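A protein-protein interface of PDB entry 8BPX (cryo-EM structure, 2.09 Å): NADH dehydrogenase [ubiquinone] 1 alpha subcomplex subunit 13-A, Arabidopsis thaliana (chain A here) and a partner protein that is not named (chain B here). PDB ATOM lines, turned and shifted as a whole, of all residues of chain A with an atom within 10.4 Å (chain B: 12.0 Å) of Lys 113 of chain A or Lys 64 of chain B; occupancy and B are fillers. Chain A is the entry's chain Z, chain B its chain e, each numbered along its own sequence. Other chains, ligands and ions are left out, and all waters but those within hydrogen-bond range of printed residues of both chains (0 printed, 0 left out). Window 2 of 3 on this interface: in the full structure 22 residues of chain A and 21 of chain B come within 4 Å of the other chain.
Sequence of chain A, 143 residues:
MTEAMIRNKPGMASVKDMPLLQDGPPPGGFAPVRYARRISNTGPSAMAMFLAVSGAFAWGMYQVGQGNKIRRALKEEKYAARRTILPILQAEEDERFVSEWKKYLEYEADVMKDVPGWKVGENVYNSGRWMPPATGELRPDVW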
ATOM      1  N   LEU A 105     -16.656  -0.688 -23.921  1.00  0.00           N
ATOM      2  CA  LEU A 105     -16.596  -0.481 -25.364  1.00  0.00           C
ATOM      3  C   LEU A 105     -16.772   0.989 -25.719  1.00  0.00           C
ATOM      4  O   LEU A 105     -16.087   1.500 -26.611  1.00  0.00           O
ATOM      5  CB  LEU A 105     -17.642  -1.342 -26.068  1.00  0.00           C
ATOM      6  CG  LEU A 105     -17.063  -2.565 -26.778  1.00  0.00           C
ATOM      7  CD1 LEU A 105     -16.074  -3.281 -25.876  1.00  0.00           C
ATOM      8  CD2 LEU A 105     -18.172  -3.506 -27.207  1.00  0.00           C
ATOM      9  N   GLU A 106     -17.683   1.686 -25.037  1.00  0.00           N
ATOM     10  CA  GLU A 106     -17.799   3.128 -25.254  1.00  0.00           C
ATOM     11  C   GLU A 106     -16.508   3.845 -24.869  1.00  0.00           C
ATOM     12  O   GLU A 106     -16.044   4.748 -25.583  1.00  0.00           O
ATOM     13  CB  GLU A 106     -18.980   3.694 -24.469  1.00  0.00           C
ATOM     14  CG  GLU A 106     -20.287   2.973 -24.701  1.00  0.00           C
ATOM     15  CD  GLU A 106     -21.176   2.981 -23.474  1.00  0.00           C
ATOM     16  OE1 GLU A 106     -20.775   3.579 -22.454  1.00  0.00           O
ATOM     17  OE2 GLU A 106     -22.276   2.395 -23.531  1.00  0.00           O
ATOM     18  N   TYR A 107     -15.908   3.445 -23.746  1.00  0.00           N
ATOM     19  CA  TYR A 107     -14.630   4.018 -23.332  1.00  0.00           C
ATOM     20  C   TYR A 107     -13.562   3.825 -24.405  1.00  0.00           C
ATOM     21  O   TYR A 107     -12.835   4.763 -24.754  1.00  0.00           O
ATOM     22  CB  TYR A 107     -14.199   3.383 -22.009  1.00  0.00           C
ATOM     23  CG  TYR A 107     -12.822   3.775 -21.526  1.00  0.00           C
ATOM     24  CD1 TYR A 107     -11.694   3.071 -21.933  1.00  0.00           C
ATOM     25  CD2 TYR A 107     -12.649   4.838 -20.655  1.00  0.00           C
ATOM     26  CE1 TYR A 107     -10.435   3.424 -21.492  1.00  0.00           C
ATOM     27  CE2 TYR A 107     -11.395   5.196 -20.207  1.00  0.00           C
ATOM     28  CZ  TYR A 107     -10.292   4.485 -20.630  1.00  0.00           C
ATOM     29  OH  TYR A 107      -9.041   4.840 -20.185  1.00  0.00           O
ATOM     30  N   GLU A 108     -13.450   2.607 -24.938  1.00  0.00           N
ATOM     31  CA  GLU A 108     -12.435   2.320 -25.947  1.00  0.00           C
ATOM     32  C   GLU A 108     -12.715   3.071 -27.243  1.00  0.00           C
ATOM     33  O   GLU A 108     -11.785   3.530 -27.917  1.00  0.00           O
ATOM     34  CB  GLU A 108     -12.360   0.814 -26.198  1.00  0.00           C
ATOM     35  CG  GLU A 108     -11.592   0.416 -27.445  1.00  0.00           C
ATOM     36  CD  GLU A 108     -11.407  -1.085 -27.563  1.00  0.00           C
ATOM     37  OE1 GLU A 108     -11.504  -1.615 -28.687  1.00  0.00           O
ATOM     38  OE2 GLU A 108     -11.169  -1.736 -26.526  1.00  0.00           O
ATOM     39  N   ALA A 109     -13.990   3.202 -27.610  1.00  0.00           N
ATOM     40  CA  ALA A 109     -14.347   3.991 -28.783  1.00  0.00           C
ATOM     41  C   ALA A 109     -13.896   5.435 -28.624  1.00  0.00           C
ATOM     42  O   ALA A 109     -13.369   6.036 -29.566  1.00  0.00           O
ATOM     43  CB  ALA A 109     -15.852   3.921 -29.022  1.00  0.00           C
ATOM     44  N   ASP A 110     -14.090   6.006 -27.434  1.00  0.00           N
ATOM     45  CA  ASP A 110     -13.640   7.375 -27.197  1.00  0.00           C
ATOM     46  C   ASP A 110     -12.119   7.475 -27.254  1.00  0.00           C
ATOM     47  O   ASP A 110     -11.571   8.327 -27.963  1.00  0.00           O
ATOM     48  CB  ASP A 110     -14.160   7.873 -25.850  1.00  0.00           C
ATOM     49  CG  ASP A 110     -13.708   9.284 -25.537  1.00  0.00           C
ATOM     50  OD1 ASP A 110     -13.488  10.069 -26.483  1.00  0.00           O
ATOM     51  OD2 ASP A 110     -13.573   9.610 -24.338  1.00  0.00           O
ATOM     52  N   VAL A 111     -11.420   6.602 -26.522  1.00  0.00           N
ATOM     53  CA  VAL A 111      -9.966   6.715 -26.407  1.00  0.00           C
ATOM     54  C   VAL A 111      -9.300   6.507 -27.760  1.00  0.00           C
ATOM     55  O   VAL A 111      -8.379   7.244 -28.136  1.00  0.00           O
ATOM     56  CB  VAL A 111      -9.430   5.723 -25.357  1.00  0.00           C
ATOM     57  CG1 VAL A 111      -7.987   5.348 -25.664  1.00  0.00           C
ATOM     58  CG2 VAL A 111      -9.538   6.308 -23.969  1.00  0.00           C
ATOM     59  N   MET A 112      -9.751   5.511 -28.515  1.00  0.00           N
ATOM     60  CA  MET A 112      -9.157   5.188 -29.803  1.00  0.00           C
ATOM     61  C   MET A 112      -9.757   5.975 -30.955  1.00  0.00           C
ATOM     62  O   MET A 112      -9.417   5.708 -32.111  1.00  0.00           O
ATOM     63  CB  MET A 112      -9.271   3.688 -30.080  1.00  0.00           C
ATOM     64  CG  MET A 112      -8.616   2.826 -29.021  1.00  0.00           C
ATOM     65  SD  MET A 112      -6.959   3.414 -28.625  1.00  0.00           S
ATOM     66  CE  MET A 112      -5.969   2.349 -29.672  1.00  0.00           C
ATOM     67  N   LYS A 113     -10.648   6.925 -30.677  1.00  0.00           N
ATOM     68  CA  LYS A 113     -11.042   7.879 -31.702  1.00  0.00           C
ATOM     69  C   LYS A 113      -9.801   8.599 -32.208  1.00  0.00           C
ATOM     70  O   LYS A 113      -8.919   8.959 -31.421  1.00  0.00           O
ATOM     71  CB  LYS A 113     -12.057   8.873 -31.142  1.00  0.00           C
ATOM     72  CG  LYS A 113     -12.600   9.858 -32.165  1.00  0.00           C
ATOM     73  CD  LYS A 113     -13.670  10.746 -31.559  1.00  0.00           C
ATOM     74  CE  LYS A 113     -14.008  11.905 -32.479  1.00  0.00           C
ATOM     75  NZ  LYS A 113     -14.949  12.865 -31.839  1.00  0.00           N
ATOM     76  N   ASP A 114      -9.712   8.759 -33.531  1.00  0.00           N
ATOM     77  CA  ASP A 114      -8.582   9.381 -34.218  1.00  0.00           C
ATOM     78  C   ASP A 114      -7.340   8.497 -34.238  1.00  0.00           C
ATOM     79  O   ASP A 114      -6.231   8.996 -34.444  1.00  0.00           O
ATOM     80  CB  ASP A 114      -8.237  10.755 -33.628  1.00  0.00           C
ATOM     81  CG  ASP A 114      -8.963  11.886 -34.324  1.00  0.00           C
ATOM     82  OD1 ASP A 114      -9.175  11.793 -35.551  1.00  0.00           O
ATOM     83  OD2 ASP A 114      -9.326  12.867 -33.642  1.00  0.00           O
ATOM     84  N   VAL A 115      -7.496   7.195 -34.030  1.00  0.00           N
ATOM     85  CA  VAL A 115      -6.444   6.220 -34.287  1.00  0.00           C
ATOM     86  C   VAL A 115      -6.871   5.405 -35.506  1.00  0.00           C
ATOM     87  O   VAL A 115      -7.770   4.557 -35.398  1.00  0.00           O
ATOM     88  CB  VAL A 115      -6.177   5.316 -33.078  1.00  0.00           C
ATOM     89  CG1 VAL A 115      -4.812   4.671 -33.206  1.00  0.00           C
ATOM     90  CG2 VAL A 115      -6.268   6.108 -31.794  1.00  0.00           C
ATOM     91  N   PRO A 116      -6.276   5.630 -36.674  1.00  0.00           N
ATOM     92  CA  PRO A 116      -6.757   4.965 -37.888  1.00  0.00           C
ATOM     93  C   PRO A 116      -6.523   3.464 -37.848  1.00  0.00           C
ATOM     94  O   PRO A 116      -5.561   2.974 -37.252  1.00  0.00           O
ATOM     95  CB  PRO A 116      -5.936   5.625 -39.000  1.00  0.00           C
ATOM     96  CG  PRO A 116      -4.678   6.051 -38.320  1.00  0.00           C
ATOM     97  CD  PRO A 116      -5.072   6.439 -36.922  1.00  0.00           C
ATOM     98  N   GLY A 117      -7.426   2.734 -38.501  1.00  0.00           N
ATOM     99  CA  GLY A 117      -7.327   1.296 -38.608  1.00  0.00           C
ATOM    100  C   GLY A 117      -7.863   0.522 -37.426  1.00  0.00           C
ATOM    101  O   GLY A 117      -7.891  -0.714 -37.479  1.00  0.00           O
ATOM    102  N   TRP A 118      -8.293   1.198 -36.366  1.00  0.00           N
ATOM    103  CA  TRP A 118      -8.807   0.508 -35.196  1.00  0.00           C
ATOM    104  C   TRP A 118     -10.176  -0.107 -35.479  1.00  0.00           C
ATOM    105  O   TRP A 118     -10.895   0.291 -36.398  1.00  0.00           O
ATOM    106  CB  TRP A 118      -8.899   1.463 -34.005  1.00  0.00           C
ATOM    107  CG  TRP A 118      -8.766   0.773 -32.691  1.00  0.00           C
ATOM    108  CD1 TRP A 118      -9.739   0.608 -31.750  1.00  0.00           C
ATOM    109  CD2 TRP A 118      -7.593   0.135 -32.173  1.00  0.00           C
ATOM    110  NE1 TRP A 118      -9.245  -0.089 -30.673  1.00  0.00           N
ATOM    111  CE2 TRP A 118      -7.929  -0.390 -30.907  1.00  0.00           C
ATOM    112  CE3 TRP A 118      -6.294  -0.042 -32.652  1.00  0.00           C
ATOM    113  CZ2 TRP A 118      -7.011  -1.079 -30.118  1.00  0.00           C
ATOM    114  CZ3 TRP A 118      -5.383  -0.727 -31.867  1.00  0.00           C
ATOM    115  CH2 TRP A 118      -5.747  -1.235 -30.614  1.00  0.00           C
ATOM    116  N   LYS A 119     -10.515  -1.111 -34.672  1.00  0.00           N
ATOM    117  CA  LYS A 119     -11.841  -1.717 -34.659  1.00  0.00           C
ATOM    118  C   LYS A 119     -12.216  -1.962 -33.209  1.00  0.00           C
ATOM    119  O   LYS A 119     -11.556  -2.748 -32.523  1.00  0.00           O
ATOM    120  CB  LYS A 119     -11.876  -3.025 -35.452  1.00  0.00           C
ATOM    121  CG  LYS A 119     -11.895  -2.851 -36.954  1.00  0.00           C
ATOM    122  CD  LYS A 119     -11.336  -4.074 -37.658  1.00  0.00           C
ATOM    123  CE  LYS A 119     -11.522  -3.975 -39.161  1.00  0.00           C
ATOM    124  NZ  LYS A 119     -12.954  -4.105 -39.544  1.00  0.00           N
ATOM    125  N   VAL A 120     -13.276  -1.301 -32.747  1.00  0.00           N
ATOM    126  CA  VAL A 120     -13.603  -1.310 -31.327  1.00  0.00           C
ATOM    127  C   VAL A 120     -14.104  -2.690 -30.924  1.00  0.00           C
ATOM    128  O   VAL A 120     -15.011  -3.250 -31.553  1.00  0.00           O
ATOM    129  CB  VAL A 120     -14.635  -0.218 -31.010  1.00  0.00           C
ATOM    130  CG1 VAL A 120     -15.242  -0.436 -29.632  1.00  0.00           C
ATOM    131  CG2 VAL A 120     -13.985   1.153 -31.101  1.00  0.00           C
ATOM    132  N   ARG B  53      -2.950  -5.443 -27.678  1.00  0.00           N
ATOM    133  CA  ARG B  53      -3.979  -4.485 -28.074  1.00  0.00           C
ATOM    134  C   ARG B  53      -4.398  -3.603 -26.900  1.00  0.00           C
ATOM    135  O   ARG B  53      -4.552  -2.378 -27.040  1.00  0.00           O
ATOM    136  CB  ARG B  53      -5.174  -5.242 -28.654  1.00  0.00           C
ATOM    137  CG  ARG B  53      -6.499  -4.515 -28.585  1.00  0.00           C
ATOM    138  CD  ARG B  53      -7.605  -5.380 -29.161  1.00  0.00           C
ATOM    139  NE  ARG B  53      -8.853  -4.644 -29.312  1.00  0.00           N
ATOM    140  CZ  ARG B  53      -9.211  -4.006 -30.417  1.00  0.00           C
ATOM    141  NH1 ARG B  53      -8.428  -3.986 -31.484  1.00  0.00           N
ATOM    142  NH2 ARG B  53     -10.378  -3.373 -30.450  1.00  0.00           N
ATOM    143  N   ASN B  55      -2.560  -2.840 -24.382  1.00  0.00           N
ATOM    144  CA  ASN B  55      -1.447  -1.933 -24.138  1.00  0.00           C
ATOM    145  C   ASN B  55      -1.422  -0.802 -25.152  1.00  0.00           C
ATOM    146  O   ASN B  55      -1.022   0.312 -24.815  1.00  0.00           O
ATOM    147  CB  ASN B  55      -0.126  -2.697 -24.157  1.00  0.00           C
ATOM    148  CG  ASN B  55       0.040  -3.603 -22.949  1.00  0.00           C
ATOM    149  OD1 ASN B  55      -0.689  -3.483 -21.966  1.00  0.00           O
ATOM    150  ND2 ASN B  55       1.004  -4.509 -23.017  1.00  0.00           N
ATOM    151  N   ARG B  56      -1.828  -1.070 -26.393  1.00  0.00           N
ATOM    152  CA  ARG B  56      -1.993   0.014 -27.359  1.00  0.00           C
ATOM    153  C   ARG B  56      -3.029   1.021 -26.875  1.00  0.00           C
ATOM    154  O   ARG B  56      -2.837   2.238 -27.004  1.00  0.00           O
ATOM    155  CB  ARG B  56      -2.393  -0.547 -28.723  1.00  0.00           C
ATOM    156  CG  ARG B  56      -1.277  -0.550 -29.732  1.00  0.00           C
ATOM    157  CD  ARG B  56      -1.715  -1.148 -31.047  1.00  0.00           C
ATOM    158  NE  ARG B  56      -0.833  -2.224 -31.479  1.00  0.00           N
ATOM    159  CZ  ARG B  56      -1.118  -3.512 -31.371  1.00  0.00           C
ATOM    160  NH1 ARG B  56      -2.267  -3.925 -30.863  1.00  0.00           N
ATOM    161  NH2 ARG B  56      -0.232  -4.410 -31.791  1.00  0.00           N
ATOM    162  N   ILE B  57      -4.135   0.528 -26.317  1.00  0.00           N
ATOM    163  CA  ILE B  57      -5.158   1.433 -25.790  1.00  0.00           C
ATOM    164  C   ILE B  57      -4.584   2.283 -24.661  1.00  0.00           C
ATOM    165  O   ILE B  57      -4.776   3.507 -24.612  1.00  0.00           O
ATOM    166  CB  ILE B  57      -6.394   0.643 -25.327  1.00  0.00           C
ATOM    167  CG1 ILE B  57      -7.176   0.120 -26.530  1.00  0.00           C
ATOM    168  CG2 ILE B  57      -7.294   1.511 -24.452  1.00  0.00           C
ATOM    169  CD1 ILE B  57      -8.063  -1.052 -26.202  1.00  0.00           C
ATOM    170  N   TYR B  58      -3.859   1.644 -23.741  1.00  0.00           N
ATOM    171  CA  TYR B  58      -3.232   2.376 -22.640  1.00  0.00           C
ATOM    172  C   TYR B  58      -2.215   3.392 -23.154  1.00  0.00           C
ATOM    173  O   TYR B  58      -2.104   4.502 -22.618  1.00  0.00           O
ATOM    174  CB  TYR B  58      -2.575   1.390 -21.674  1.00  0.00           C
ATOM    175  CG  TYR B  58      -1.471   1.973 -20.819  1.00  0.00           C
ATOM    176  CD1 TYR B  58      -1.758   2.663 -19.650  1.00  0.00           C
ATOM    177  CD2 TYR B  58      -0.138   1.824 -21.178  1.00  0.00           C
ATOM    178  CE1 TYR B  58      -0.751   3.192 -18.869  1.00  0.00           C
ATOM    179  CE2 TYR B  58       0.874   2.351 -20.402  1.00  0.00           C
ATOM    180  CZ  TYR B  58       0.565   3.031 -19.251  1.00  0.00           C
ATOM    181  OH  TYR B  58       1.576   3.555 -18.480  1.00  0.00           O
ATOM    182  N   LYS B  59      -1.460   3.021 -24.189  1.00  0.00           N
ATOM    183  CA  LYS B  59      -0.480   3.917 -24.792  1.00  0.00           C
ATOM    184  C   LYS B  59      -1.150   5.160 -25.354  1.00  0.00           C
ATOM    185  O   LYS B  59      -0.687   6.284 -25.133  1.00  0.00           O
ATOM    186  CB  LYS B  59       0.269   3.179 -25.899  1.00  0.00           C
ATOM    187  CG  LYS B  59       1.592   3.788 -26.302  1.00  0.00           C
ATOM    188  CD  LYS B  59       2.539   2.721 -26.830  1.00  0.00           C
ATOM    189  CE  LYS B  59       2.312   1.379 -26.151  1.00  0.00           C
ATOM    190  NZ  LYS B  59       3.407   0.423 -26.456  1.00  0.00           N
ATOM    191  N   GLU B  60      -2.236   4.974 -26.105  1.00  0.00           N
ATOM    192  CA  GLU B  60      -2.941   6.119 -26.669  1.00  0.00           C
ATOM    193  C   GLU B  60      -3.536   6.991 -25.569  1.00  0.00           C
ATOM    194  O   GLU B  60      -3.559   8.223 -25.683  1.00  0.00           O
ATOM    195  CB  GLU B  60      -4.021   5.645 -27.639  1.00  0.00           C
ATOM    196  CG  GLU B  60      -4.784   6.774 -28.305  1.00  0.00           C
ATOM    197  CD  GLU B  60      -4.029   7.360 -29.481  1.00  0.00           C
ATOM    198  OE1 GLU B  60      -3.376   6.590 -30.216  1.00  0.00           O
ATOM    199  OE2 GLU B  60      -4.088   8.593 -29.670  1.00  0.00           O
ATOM    200  N   GLU B  61      -4.010   6.368 -24.487  1.00  0.00           N
ATOM    201  CA  GLU B  61      -4.496   7.151 -23.355  1.00  0.00           C
ATOM    202  C   GLU B  61      -3.383   7.994 -22.748  1.00  0.00           C
ATOM    203  O   GLU B  61      -3.596   9.162 -22.402  1.00  0.00           O
ATOM    204  CB  GLU B  61      -5.106   6.235 -22.295  1.00  0.00           C
ATOM    205  CG  GLU B  61      -6.082   6.939 -21.376  1.00  0.00           C
ATOM    206  CD  GLU B  61      -6.374   6.149 -20.117  1.00  0.00           C
ATOM    207  OE1 GLU B  61      -5.592   5.231 -19.793  1.00  0.00           O
ATOM    208  OE2 GLU B  61      -7.386   6.447 -19.450  1.00  0.00           O
ATOM    209  N   GLN B  62      -2.185   7.423 -22.611  1.00  0.00           N
ATOM    210  CA  GLN B  62      -1.073   8.184 -22.050  1.00  0.00           C
ATOM    211  C   GLN B  62      -0.589   9.263 -23.011  1.00  0.00           C
ATOM    212  O   GLN B  62      -0.047  10.284 -22.576  1.00  0.00           O
ATOM    213  CB  GLN B  62       0.077   7.246 -21.683  1.00  0.00           C
ATOM    214  CG  GLN B  62       0.655   7.454 -20.289  1.00  0.00           C
ATOM    215  CD  GLN B  62      -0.378   7.296 -19.183  1.00  0.00           C
ATOM    216  OE1 GLN B  62      -1.398   6.630 -19.356  1.00  0.00           O
ATOM    217  NE2 GLN B  62      -0.112   7.910 -18.037  1.00  0.00           N
ATOM    218  N   ARG B  63      -0.764   9.048 -24.315  1.00  0.00           N
ATOM    219  CA  ARG B  63      -0.353  10.044 -25.297  1.00  0.00           C
ATOM    220  C   ARG B  63      -1.311  11.230 -25.325  1.00  0.00           C
ATOM    221  O   ARG B  63      -0.878  12.380 -25.465  1.00  0.00           O
ATOM    222  CB  ARG B  63      -0.251   9.402 -26.679  1.00  0.00           C
ATOM    223  CG  ARG B  63       0.391  10.279 -27.723  1.00  0.00           C
ATOM    224  CD  ARG B  63       0.112   9.763 -29.123  1.00  0.00           C
ATOM    225  NE  ARG B  63      -1.296   9.863 -29.479  1.00  0.00           N
ATOM    226  CZ  ARG B  63      -1.881  10.968 -29.918  1.00  0.00           C
ATOM    227  NH1 ARG B  63      -1.207  12.100 -30.052  1.00  0.00           N
ATOM    228  NH2 ARG B  63      -3.172  10.938 -30.235  1.00  0.00           N
ATOM    229  N   LYS B  64      -2.615  10.977 -25.188  1.00  0.00           N
ATOM    230  CA  LYS B  64      -3.618  12.038 -25.230  1.00  0.00           C
ATOM    231  C   LYS B  64      -3.900  12.642 -23.859  1.00  0.00           C
ATOM    232  O   LYS B  64      -5.012  13.139 -23.625  1.00  0.00           O
ATOM    233  CB  LYS B  64      -4.915  11.521 -25.850  1.00  0.00           C
ATOM    234  CG  LYS B  64      -4.823  11.170 -27.316  1.00  0.00           C
ATOM    235  CD  LYS B  64      -6.184  10.759 -27.854  1.00  0.00           C
ATOM    236  CE  LYS B  64      -6.358  11.179 -29.305  1.00  0.00           C
ATOM    237  NZ  LYS B  64      -7.794  11.312 -29.672  1.00  0.00           N
ATOM    238  N   LEU B  65      -2.936  12.617 -22.945  1.00  0.00           N
ATOM    239  CA  LEU B  65      -3.145  13.162 -21.609  1.00  0.00           C
ATOM    240  C   LEU B  65      -1.915  13.914 -21.112  1.00  0.00           C
ATOM    241  O   LEU B  65      -0.810  13.377 -21.103  1.00  0.00           O
ATOM    242  CB  LEU B  65      -3.508  12.048 -20.627  1.00  0.00           C
ATOM    243  CG  LEU B  65      -3.580  12.443 -19.152  1.00  0.00           C
ATOM    244  CD1 LEU B  65      -4.675  13.475 -18.920  1.00  0.00           C
ATOM    245  CD2 LEU B  65      -3.793  11.220 -18.273  1.00  0.00           C
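NH2 of Arg 53 of chain B lies close to NE1 of Trp 118 of chain A (3.5 Å). The side-chain carboxylate of Glu 108 of chain A lies within salt-bridge range of the guanidinium group of Arg 53 of chain B (2.7 Å). The backbone carbonyl oxygen of Lys 113 of chain A lies within hydrogen-bond range of the side-chain amino group of Lys 64 of chain B (3.1 Å). The side-chain carboxylate (OE2) of Glu 61 of chain B lies within hydrogen-bond range of the side-chain hydroxyl (OH) of Tyr 107 of chain A, 2.4 Å away. The backbone carbonyl oxygen of Lys 119 of chain A lies within hydrogen-bond range of the guanidinium group of Arg 53 of chain B.
The side-chain carboxylate (OE2) of Glu 60 of chain B is in salt-bridge range of the guanidinium group (NH2) of Arg 63 of chain B, at 2.6 Å. The indole nitrogen of Trp 118 of chain A lies within hydrogen-bond range of the side-chain carboxylate of Glu 108 of chain A (3.4 Å).
Among the printed residues, pairs that only touch across the chains: Glu 108 of chain A with Ile 57 of chain B (3.2 Å), Val 115 of chain A with Glu 60 of chain B (3.3 Å), Val 111 of chain A with Glu 60 of chain B (3.6 Å), Trp 118 of chain A with Arg 56 of chain B (3.8 Å), Trp 118 of chain A with Ile 57 of chain B (3.8 Å), Val 120 of chain A with Arg 53 of chain B (3.8 Å), Met 112 of chain A with Glu 60 of chain B (3.8 Å), Val 111 of chain A with Ile 57 of chain B (3.8 Å) and Met 112 of chain A with Ile 57 of chain B (3.9 Å).
Lys 113 of chain A touches just one residue of chain B: Lys 64 (3.1 Å). Printed residues of chain A within 4 Å of Lys 64 of chain B: Lys 113 (3.1 Å). No residue of chain B comes within 4 Å of Ala 109 of chain A. Val 111 of chain A touches just these residues of chain B: Ile 57 and Glu 60. Met 112 of chain A touches just these residues of chain B: Ile 57 and Glu 60. Val 115 of chain A touches just one residue of chain B: Glu 60 (3.3 Å). Of chain A, only Val 111 (3.6 Å), Met 112 (3.8 Å) and Val 115 (3.3 Å) come within 4 Å of Glu 60 of chain B. No residue of chain A comes within 4 Å of Arg 63 of chain B. No residue of chain A comes within 4 Å of Leu 65 of chain B. Of the printed residues of chain A, Arg 53 of chain B touches Glu 108 (2.7 Å), Trp 118 (3.5 Å), Lys 119 (2.5 Å) and Val 120 (3.8 Å). Printed residues of chain B within 4 Å of Trp 118 of chain A: Arg 53 (3.5 Å), Arg 56 (3.8 Å) and Ile 57 (3.8 Å). Of the printed residues of chain B, Val 120 of chain A touches Arg 53 (3.8 Å). Tyr 58 of chain B touches none of the printed residues of chain A. The nearest residue of chain B that does not touch Lys 113 of chain A is Glu 60 of chain B (5.2 Å). The nearest printed residue of chain B that does not touch Glu 108 of chain A is Glu 60 of chain B (7.7 Å).
Of the 16 printed residues of chain A, 9 touch a printed residue of chain B. Hydrophobic or aromatic side chains of chain A within 4 Å of the printed part of chain B: Tyr 107, Val 111, Met 112, Val 115 and Trp 118. Among the printed residues, 14 pairs touch across the chains.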
